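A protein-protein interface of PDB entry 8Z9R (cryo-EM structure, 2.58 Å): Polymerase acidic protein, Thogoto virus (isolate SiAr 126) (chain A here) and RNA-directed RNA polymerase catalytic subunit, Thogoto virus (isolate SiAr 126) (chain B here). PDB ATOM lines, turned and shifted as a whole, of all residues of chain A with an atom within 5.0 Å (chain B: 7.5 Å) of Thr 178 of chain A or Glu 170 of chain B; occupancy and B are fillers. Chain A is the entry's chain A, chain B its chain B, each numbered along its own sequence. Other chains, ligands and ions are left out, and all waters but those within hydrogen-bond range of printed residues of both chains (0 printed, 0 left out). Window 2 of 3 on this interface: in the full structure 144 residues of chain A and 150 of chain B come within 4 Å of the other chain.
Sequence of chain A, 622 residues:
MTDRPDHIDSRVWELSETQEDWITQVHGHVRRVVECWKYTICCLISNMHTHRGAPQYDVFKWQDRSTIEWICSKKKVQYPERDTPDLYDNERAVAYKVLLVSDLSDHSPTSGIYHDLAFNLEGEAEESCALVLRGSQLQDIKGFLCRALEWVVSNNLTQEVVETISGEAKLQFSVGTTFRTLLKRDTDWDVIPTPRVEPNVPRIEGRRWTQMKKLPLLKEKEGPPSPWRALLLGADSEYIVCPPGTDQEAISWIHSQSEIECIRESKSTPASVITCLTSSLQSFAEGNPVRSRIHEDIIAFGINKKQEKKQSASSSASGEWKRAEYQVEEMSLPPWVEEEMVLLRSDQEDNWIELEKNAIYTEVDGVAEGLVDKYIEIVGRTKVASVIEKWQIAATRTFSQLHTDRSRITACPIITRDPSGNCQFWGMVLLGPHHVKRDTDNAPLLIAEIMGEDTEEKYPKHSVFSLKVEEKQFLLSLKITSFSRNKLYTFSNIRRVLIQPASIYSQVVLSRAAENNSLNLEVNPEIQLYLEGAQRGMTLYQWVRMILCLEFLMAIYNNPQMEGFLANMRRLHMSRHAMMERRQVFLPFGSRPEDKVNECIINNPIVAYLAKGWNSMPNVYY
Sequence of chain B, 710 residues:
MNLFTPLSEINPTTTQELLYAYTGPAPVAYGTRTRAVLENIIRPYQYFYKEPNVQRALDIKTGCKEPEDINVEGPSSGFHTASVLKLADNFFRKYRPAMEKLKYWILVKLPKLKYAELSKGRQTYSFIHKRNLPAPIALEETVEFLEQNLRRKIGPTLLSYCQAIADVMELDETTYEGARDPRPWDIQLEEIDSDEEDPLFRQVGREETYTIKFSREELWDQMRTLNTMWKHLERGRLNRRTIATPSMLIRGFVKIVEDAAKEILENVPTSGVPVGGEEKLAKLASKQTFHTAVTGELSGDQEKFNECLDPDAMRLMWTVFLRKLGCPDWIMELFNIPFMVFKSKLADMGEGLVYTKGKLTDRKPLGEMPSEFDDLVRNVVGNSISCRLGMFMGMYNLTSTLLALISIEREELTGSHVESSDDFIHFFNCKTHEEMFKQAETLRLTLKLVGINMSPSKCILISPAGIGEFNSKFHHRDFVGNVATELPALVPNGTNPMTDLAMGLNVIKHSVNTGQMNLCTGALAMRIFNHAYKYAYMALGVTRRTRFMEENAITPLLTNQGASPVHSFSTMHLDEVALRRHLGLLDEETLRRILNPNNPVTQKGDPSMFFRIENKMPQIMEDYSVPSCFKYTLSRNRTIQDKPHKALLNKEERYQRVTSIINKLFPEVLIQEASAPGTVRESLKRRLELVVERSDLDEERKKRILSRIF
The side-chain hydroxyl (OG1) of Thr 178 of chain A lies close to the guanidinium group (NE) of Arg 216 of chain B (3.3 Å).
The side-chain carboxylate of Glu 170 of chain B sits at hydrogen-bond distance from the backbone NH of Thr 177 of chain A (3.2 Å).
The backbone NH (N) of Phe 179 of chain A is in hydrogen-bond range of the side-chain carboxylate (OE2) of Glu 170 of chain B, at 3.1 Å.
The guanidinium group (NE) of Arg 216 of chain B lies within hydrogen-bond range of the backbone carbonyl oxygen (O) of Leu 171 of chain B.
The backbone carbonyl oxygen of Thr 178 of chain A is in hydrogen-bond range of the side-chain hydroxyl of Thr 181 of chain A (2.4 Å).
The backbone carbonyl oxygen (O) of Glu 170 of chain B is in hydrogen-bond range of the guanidinium group (NH2) of Arg 216 of chain B.
OD1 of Asp 172 of chain B is in salt-bridge range of NH2 of Arg 216 of chain B, at 2.7 Å.
O of Met 169 of chain B is in hydrogen-bond range of NE of Arg 216 of chain B.
Among the printed residues, pairs that only touch across the chains: Gly 176 of chain A with Glu 170 of chain B, Thr 178 of chain A with Glu 170 of chain B, Phe 179 of chain A with Met 169 of chain B, Leu 182 of chain A with Glu 217 of chain B, Thr 178 of chain A with Met 169 of chain B and Leu 182 of chain A with Arg 216 of chain B.
Of the printed residues of chain B, Gly 176 of chain A touches Glu 170 (3.1 Å).
Of the printed residues of chain B, Thr 178 of chain A touches Met 169 (3.9 Å), Glu 170 (3.3 Å) and Arg 216 (3.3 Å).
Of the printed residues of chain B, Leu 182 of chain A touches Arg 216 and Glu 217.
Printed residues of chain A within 4 Å of Met 169 of chain B: Thr 178 (3.9 Å) and Phe 179 (3.5 Å).
Glu 170 of chain B touches just these residues of chain A: Gly 176 (3.1 Å), Thr 177 (3.2 Å), Thr 178 (3.3 Å) and Phe 179 (3.1 Å).
Of the printed residues of chain A, Arg 216 of chain B touches Thr 178 (3.3 Å) and Leu 182 (3.9 Å).
Of the printed residues of chain A, Glu 217 of chain B touches Leu 182 (3.6 Å).
The nearest residue of chain A that does not touch Glu 170 of chain B is Arg 180 of chain A (4.8 Å).
The nearest printed residue of chain B that does not touch Leu 182 of chain A is Met 169 of chain B (4.7 Å).
Hydrophobic or aromatic side chains of chain B that line the printed part of chain A: Met 169.
Hydrophobic or aromatic side chains of chain A that line the printed part of chain B: Phe 179 and Leu 182.
Among the printed residues, no Asp or Glu carboxylate lies within 4 Å of a Lys or Arg side-chain nitrogen of the other chain.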
ATOM      1  N   VAL A 175     -17.192   3.831 -20.310  1.00  0.00           N
ATOM      2  CA  VAL A 175     -18.585   3.498 -20.585  1.00  0.00           C
ATOM      3  C   VAL A 175     -18.612   2.457 -21.693  1.00  0.00           C
ATOM      4  O   VAL A 175     -17.984   2.642 -22.743  1.00  0.00           O
ATOM      5  CB  VAL A 175     -19.398   4.742 -20.979  1.00  0.00           C
ATOM      6  CG1 VAL A 175     -20.856   4.378 -21.192  1.00  0.00           C
ATOM      7  CG2 VAL A 175     -19.265   5.819 -19.917  1.00  0.00           C
ATOM      8  N   GLY A 176     -19.337   1.366 -21.463  1.00  0.00           N
ATOM      9  CA  GLY A 176     -19.413   0.292 -22.433  1.00  0.00           C
ATOM     10  C   GLY A 176     -20.251   0.627 -23.649  1.00  0.00           C
ATOM     11  O   GLY A 176     -20.450   1.801 -23.972  1.00  0.00           O
ATOM     12  N   THR A 177     -20.751  -0.402 -24.334  1.00  0.00           N
ATOM     13  CA  THR A 177     -21.512  -0.201 -25.564  1.00  0.00           C
ATOM     14  C   THR A 177     -23.013  -0.133 -25.299  1.00  0.00           C
ATOM     15  O   THR A 177     -23.666   0.854 -25.654  1.00  0.00           O
ATOM     16  CB  THR A 177     -21.196  -1.317 -26.566  1.00  0.00           C
ATOM     17  OG1 THR A 177     -21.593  -2.580 -26.018  1.00  0.00           O
ATOM     18  CG2 THR A 177     -19.709  -1.347 -26.877  1.00  0.00           C
ATOM     19  N   THR A 178     -23.576  -1.176 -24.682  1.00  0.00           N
ATOM     20  CA  THR A 178     -25.017  -1.204 -24.457  1.00  0.00           C
ATOM     21  C   THR A 178     -25.457  -0.134 -23.465  1.00  0.00           C
ATOM     22  O   THR A 178     -26.564   0.404 -23.589  1.00  0.00           O
ATOM     23  CB  THR A 178     -25.455  -2.594 -23.988  1.00  0.00           C
ATOM     24  OG1 THR A 178     -26.876  -2.613 -23.802  1.00  0.00           O
ATOM     25  CG2 THR A 178     -24.769  -2.978 -22.689  1.00  0.00           C
ATOM     26  N   PHE A 179     -24.612   0.194 -22.486  1.00  0.00           N
ATOM     27  CA  PHE A 179     -24.931   1.291 -21.578  1.00  0.00           C
ATOM     28  C   PHE A 179     -24.978   2.615 -22.326  1.00  0.00           C
ATOM     29  O   PHE A 179     -25.823   3.470 -22.040  1.00  0.00           O
ATOM     30  CB  PHE A 179     -23.913   1.340 -20.439  1.00  0.00           C
ATOM     31  CG  PHE A 179     -24.224   2.367 -19.389  1.00  0.00           C
ATOM     32  CD1 PHE A 179     -25.527   2.583 -18.976  1.00  0.00           C
ATOM     33  CD2 PHE A 179     -23.210   3.100 -18.798  1.00  0.00           C
ATOM     34  CE1 PHE A 179     -25.814   3.522 -18.006  1.00  0.00           C
ATOM     35  CE2 PHE A 179     -23.491   4.039 -17.826  1.00  0.00           C
ATOM     36  CZ  PHE A 179     -24.795   4.249 -17.429  1.00  0.00           C
ATOM     37  N   ARG A 180     -24.081   2.800 -23.296  1.00  0.00           N
ATOM     38  CA  ARG A 180     -24.119   3.998 -24.125  1.00  0.00           C
ATOM     39  C   ARG A 180     -25.410   4.068 -24.932  1.00  0.00           C
ATOM     40  O   ARG A 180     -26.008   5.141 -25.071  1.00  0.00           O
ATOM     41  CB  ARG A 180     -22.901   4.028 -25.047  1.00  0.00           C
ATOM     42  CG  ARG A 180     -22.686   5.343 -25.766  1.00  0.00           C
ATOM     43  CD  ARG A 180     -21.421   5.291 -26.604  1.00  0.00           C
ATOM     44  NE  ARG A 180     -20.270   4.878 -25.811  1.00  0.00           N
ATOM     45  CZ  ARG A 180     -19.384   5.711 -25.285  1.00  0.00           C
ATOM     46  NH1 ARG A 180     -19.474   7.019 -25.463  1.00  0.00           N
ATOM     47  NH2 ARG A 180     -18.381   5.221 -24.562  1.00  0.00           N
ATOM     48  N   THR A 181     -25.853   2.931 -25.476  1.00  0.00           N
ATOM     49  CA  THR A 181     -27.114   2.906 -26.210  1.00  0.00           C
ATOM     50  C   THR A 181     -28.287   3.243 -25.300  1.00  0.00           C
ATOM     51  O   THR A 181     -29.207   3.965 -25.703  1.00  0.00           O
ATOM     52  CB  THR A 181     -27.321   1.540 -26.863  1.00  0.00           C
ATOM     53  OG1 THR A 181     -27.486   0.542 -25.848  1.00  0.00           O
ATOM     54  CG2 THR A 181     -26.130   1.181 -27.734  1.00  0.00           C
ATOM     55  N   LEU A 182     -28.279   2.724 -24.070  1.00  0.00           N
ATOM     56  CA  LEU A 182     -29.328   3.075 -23.116  1.00  0.00           C
ATOM     57  C   LEU A 182     -29.308   4.564 -22.800  1.00  0.00           C
ATOM     58  O   LEU A 182     -30.363   5.200 -22.698  1.00  0.00           O
ATOM     59  CB  LEU A 182     -29.169   2.262 -21.832  1.00  0.00           C
ATOM     60  CG  LEU A 182     -29.430   0.757 -21.897  1.00  0.00           C
ATOM     61  CD1 LEU A 182     -29.077   0.105 -20.573  1.00  0.00           C
ATOM     62  CD2 LEU A 182     -30.874   0.480 -22.257  1.00  0.00           C
ATOM     63  N   LEU B 150     -20.859  -8.488 -10.143  1.00  0.00           N
ATOM     64  CA  LEU B 150     -19.590  -8.354 -10.842  1.00  0.00           C
ATOM     65  C   LEU B 150     -18.537  -9.338 -10.358  1.00  0.00           C
ATOM     66  O   LEU B 150     -17.445  -9.383 -10.936  1.00  0.00           O
ATOM     67  CB  LEU B 150     -19.053  -6.926 -10.697  1.00  0.00           C
ATOM     68  CG  LEU B 150     -19.864  -5.836 -11.394  1.00  0.00           C
ATOM     69  CD1 LEU B 150     -19.365  -4.463 -10.988  1.00  0.00           C
ATOM     70  CD2 LEU B 150     -19.802  -6.009 -12.900  1.00  0.00           C
ATOM     71  N   GLN B 163     -17.734   3.159 -11.626  1.00  0.00           N
ATOM     72  CA  GLN B 163     -17.319   2.192 -12.635  1.00  0.00           C
ATOM     73  C   GLN B 163     -18.058   0.873 -12.465  1.00  0.00           C
ATOM     74  O   GLN B 163     -18.436   0.236 -13.452  1.00  0.00           O
ATOM     75  CB  GLN B 163     -15.809   1.975 -12.570  1.00  0.00           C
ATOM     76  CG  GLN B 163     -15.291   0.986 -13.596  1.00  0.00           C
ATOM     77  CD  GLN B 163     -15.614   1.404 -15.014  1.00  0.00           C
ATOM     78  OE1 GLN B 163     -15.193   2.464 -15.471  1.00  0.00           O
ATOM     79  NE2 GLN B 163     -16.370   0.574 -15.719  1.00  0.00           N
ATOM     80  N   ALA B 164     -18.271   0.444 -11.221  1.00  0.00           N
ATOM     81  CA  ALA B 164     -19.061  -0.759 -10.978  1.00  0.00           C
ATOM     82  C   ALA B 164     -20.500  -0.578 -11.444  1.00  0.00           C
ATOM     83  O   ALA B 164     -21.090  -1.493 -12.035  1.00  0.00           O
ATOM     84  CB  ALA B 164     -19.022  -1.117  -9.495  1.00  0.00           C
ATOM     85  N   ILE B 165     -21.080   0.596 -11.182  1.00  0.00           N
ATOM     86  CA  ILE B 165     -22.436   0.877 -11.650  1.00  0.00           C
ATOM     87  C   ILE B 165     -22.503   0.781 -13.168  1.00  0.00           C
ATOM     88  O   ILE B 165     -23.435   0.194 -13.730  1.00  0.00           O
ATOM     89  CB  ILE B 165     -22.900   2.260 -11.156  1.00  0.00           C
ATOM     90  CG1 ILE B 165     -23.009   2.291  -9.632  1.00  0.00           C
ATOM     91  CG2 ILE B 165     -24.235   2.615 -11.770  1.00  0.00           C
ATOM     92  CD1 ILE B 165     -24.113   1.438  -9.085  1.00  0.00           C
ATOM     93  N   ALA B 166     -21.514   1.356 -13.855  1.00  0.00           N
ATOM     94  CA  ALA B 166     -21.491   1.297 -15.313  1.00  0.00           C
ATOM     95  C   ALA B 166     -21.275  -0.127 -15.812  1.00  0.00           C
ATOM     96  O   ALA B 166     -21.822  -0.517 -16.850  1.00  0.00           O
ATOM     97  CB  ALA B 166     -20.407   2.226 -15.857  1.00  0.00           C
ATOM     98  N   ASP B 167     -20.474  -0.915 -15.093  1.00  0.00           N
ATOM     99  CA  ASP B 167     -20.186  -2.280 -15.521  1.00  0.00           C
ATOM    100  C   ASP B 167     -21.406  -3.179 -15.377  1.00  0.00           C
ATOM    101  O   ASP B 167     -21.640  -4.052 -16.219  1.00  0.00           O
ATOM    102  CB  ASP B 167     -19.011  -2.842 -14.722  1.00  0.00           C
ATOM    103  CG  ASP B 167     -17.672  -2.340 -15.220  1.00  0.00           C
ATOM    104  OD1 ASP B 167     -17.635  -1.713 -16.300  1.00  0.00           O
ATOM    105  OD2 ASP B 167     -16.656  -2.570 -14.534  1.00  0.00           O
ATOM    106  N   VAL B 168     -22.188  -2.990 -14.312  1.00  0.00           N
ATOM    107  CA  VAL B 168     -23.394  -3.796 -14.133  1.00  0.00           C
ATOM    108  C   VAL B 168     -24.392  -3.527 -15.251  1.00  0.00           C
ATOM    109  O   VAL B 168     -25.131  -4.428 -15.668  1.00  0.00           O
ATOM    110  CB  VAL B 168     -24.004  -3.539 -12.741  1.00  0.00           C
ATOM    111  CG1 VAL B 168     -25.355  -4.215 -12.608  1.00  0.00           C
ATOM    112  CG2 VAL B 168     -23.068  -4.047 -11.667  1.00  0.00           C
ATOM    113  N   MET B 169     -24.421  -2.296 -15.769  1.00  0.00           N
ATOM    114  CA  MET B 169     -25.315  -1.968 -16.873  1.00  0.00           C
ATOM    115  C   MET B 169     -25.009  -2.776 -18.127  1.00  0.00           C
ATOM    116  O   MET B 169     -25.877  -2.899 -18.999  1.00  0.00           O
ATOM    117  CB  MET B 169     -25.225  -0.477 -17.194  1.00  0.00           C
ATOM    118  CG  MET B 169     -26.112   0.425 -16.347  1.00  0.00           C
ATOM    119  SD  MET B 169     -27.774  -0.205 -16.053  1.00  0.00           S
ATOM    120  CE  MET B 169     -27.600  -0.807 -14.379  1.00  0.00           C
ATOM    121  N   GLU B 170     -23.799  -3.324 -18.244  1.00  0.00           N
ATOM    122  CA  GLU B 170     -23.416  -4.112 -19.407  1.00  0.00           C
ATOM    123  C   GLU B 170     -23.921  -5.547 -19.352  1.00  0.00           C
ATOM    124  O   GLU B 170     -23.906  -6.229 -20.381  1.00  0.00           O
ATOM    125  CB  GLU B 170     -21.894  -4.110 -19.556  1.00  0.00           C
ATOM    126  CG  GLU B 170     -21.318  -2.747 -19.877  1.00  0.00           C
ATOM    127  CD  GLU B 170     -21.649  -2.301 -21.283  1.00  0.00           C
ATOM    128  OE1 GLU B 170     -21.556  -3.133 -22.209  1.00  0.00           O
ATOM    129  OE2 GLU B 170     -22.022  -1.125 -21.461  1.00  0.00           O
ATOM    130  N   LEU B 171     -24.361  -6.018 -18.190  1.00  0.00           N
ATOM    131  CA  LEU B 171     -24.831  -7.386 -18.054  1.00  0.00           C
ATOM    132  C   LEU B 171     -26.234  -7.537 -18.636  1.00  0.00           C
ATOM    133  O   LEU B 171     -26.990  -6.572 -18.768  1.00  0.00           O
ATOM    134  CB  LEU B 171     -24.826  -7.818 -16.586  1.00  0.00           C
ATOM    135  CG  LEU B 171     -23.522  -8.322 -15.960  1.00  0.00           C
ATOM    136  CD1 LEU B 171     -22.414  -7.286 -16.025  1.00  0.00           C
ATOM    137  CD2 LEU B 171     -23.763  -8.749 -14.522  1.00  0.00           C
ATOM    138  N   ASP B 172     -26.572  -8.776 -18.990  1.00  0.00           N
ATOM    139  CA  ASP B 172     -27.899  -9.095 -19.502  1.00  0.00           C
ATOM    140  C   ASP B 172     -28.887  -9.397 -18.383  1.00  0.00           C
ATOM    141  O   ASP B 172     -30.030  -8.929 -18.423  1.00  0.00           O
ATOM    142  CB  ASP B 172     -27.822 -10.287 -20.458  1.00  0.00           C
ATOM    143  CG  ASP B 172     -27.312  -9.902 -21.830  1.00  0.00           C
ATOM    144  OD1 ASP B 172     -27.591  -8.770 -22.273  1.00  0.00           O
ATOM    145  OD2 ASP B 172     -26.628 -10.731 -22.466  1.00  0.00           O
ATOM    146  N   GLU B 173     -28.467 -10.174 -17.390  1.00  0.00           N
ATOM    147  CA  GLU B 173     -29.295 -10.526 -16.248  1.00  0.00           C
ATOM    148  C   GLU B 173     -28.497 -10.312 -14.972  1.00  0.00           C
ATOM    149  O   GLU B 173     -27.331 -10.706 -14.886  1.00  0.00           O
ATOM    150  CB  GLU B 173     -29.769 -11.985 -16.325  1.00  0.00           C
ATOM    151  CG  GLU B 173     -30.719 -12.287 -17.472  1.00  0.00           C
ATOM    152  CD  GLU B 173     -32.056 -11.588 -17.322  1.00  0.00           C
ATOM    153  OE1 GLU B 173     -32.497 -11.388 -16.170  1.00  0.00           O
ATOM    154  OE2 GLU B 173     -32.669 -11.242 -18.355  1.00  0.00           O
ATOM    155  N   THR B 174     -29.129  -9.685 -13.985  1.00  0.00           N
ATOM    156  CA  THR B 174     -28.520  -9.481 -12.680  1.00  0.00           C
ATOM    157  C   THR B 174     -29.457 -10.003 -11.601  1.00  0.00           C
ATOM    158  O   THR B 174     -30.682  -9.965 -11.746  1.00  0.00           O
ATOM    159  CB  THR B 174     -28.192  -8.003 -12.423  1.00  0.00           C
ATOM    160  OG1 THR B 174     -29.392  -7.226 -12.483  1.00  0.00           O
ATOM    161  CG2 THR B 174     -27.206  -7.486 -13.458  1.00  0.00           C
ATOM    162  N   ARG B 216     -31.655  -6.118 -18.133  1.00  0.00           N
ATOM    163  CA  ARG B 216     -31.017  -4.840 -18.422  1.00  0.00           C
ATOM    164  C   ARG B 216     -32.045  -3.720 -18.481  1.00  0.00           C
ATOM    165  O   ARG B 216     -31.816  -2.629 -17.946  1.00  0.00           O
ATOM    166  CB  ARG B 216     -30.233  -4.910 -19.731  1.00  0.00           C
ATOM    167  CG  ARG B 216     -29.246  -3.763 -19.889  1.00  0.00           C
ATOM    168  CD  ARG B 216     -28.554  -3.784 -21.239  1.00  0.00           C
ATOM    169  NE  ARG B 216     -27.392  -4.663 -21.246  1.00  0.00           N
ATOM    170  CZ  ARG B 216     -27.311  -5.789 -21.937  1.00  0.00           C
ATOM    171  NH1 ARG B 216     -28.311  -6.210 -22.693  1.00  0.00           N
ATOM    172  NH2 ARG B 216     -26.197  -6.514 -21.868  1.00  0.00           N
ATOM    173  N   GLU B 217     -33.190  -3.972 -19.118  1.00  0.00           N
ATOM    174  CA  GLU B 217     -34.231  -2.952 -19.197  1.00  0.00           C
ATOM    175  C   GLU B 217     -34.835  -2.664 -17.829  1.00  0.00           C
ATOM    176  O   GLU B 217     -35.075  -1.501 -17.487  1.00  0.00           O
ATOM    177  CB  GLU B 217     -35.315  -3.384 -20.183  1.00  0.00           C
ATOM    178  CG  GLU B 217     -34.876  -3.381 -21.643  1.00  0.00           C
ATOM    179  CD  GLU B 217     -34.048  -2.164 -22.015  1.00  0.00           C
ATOM    180  OE1 GLU B 217     -34.441  -1.034 -21.655  1.00  0.00           O
ATOM    181  OE2 GLU B 217     -32.999  -2.339 -22.669  1.00  0.00           O
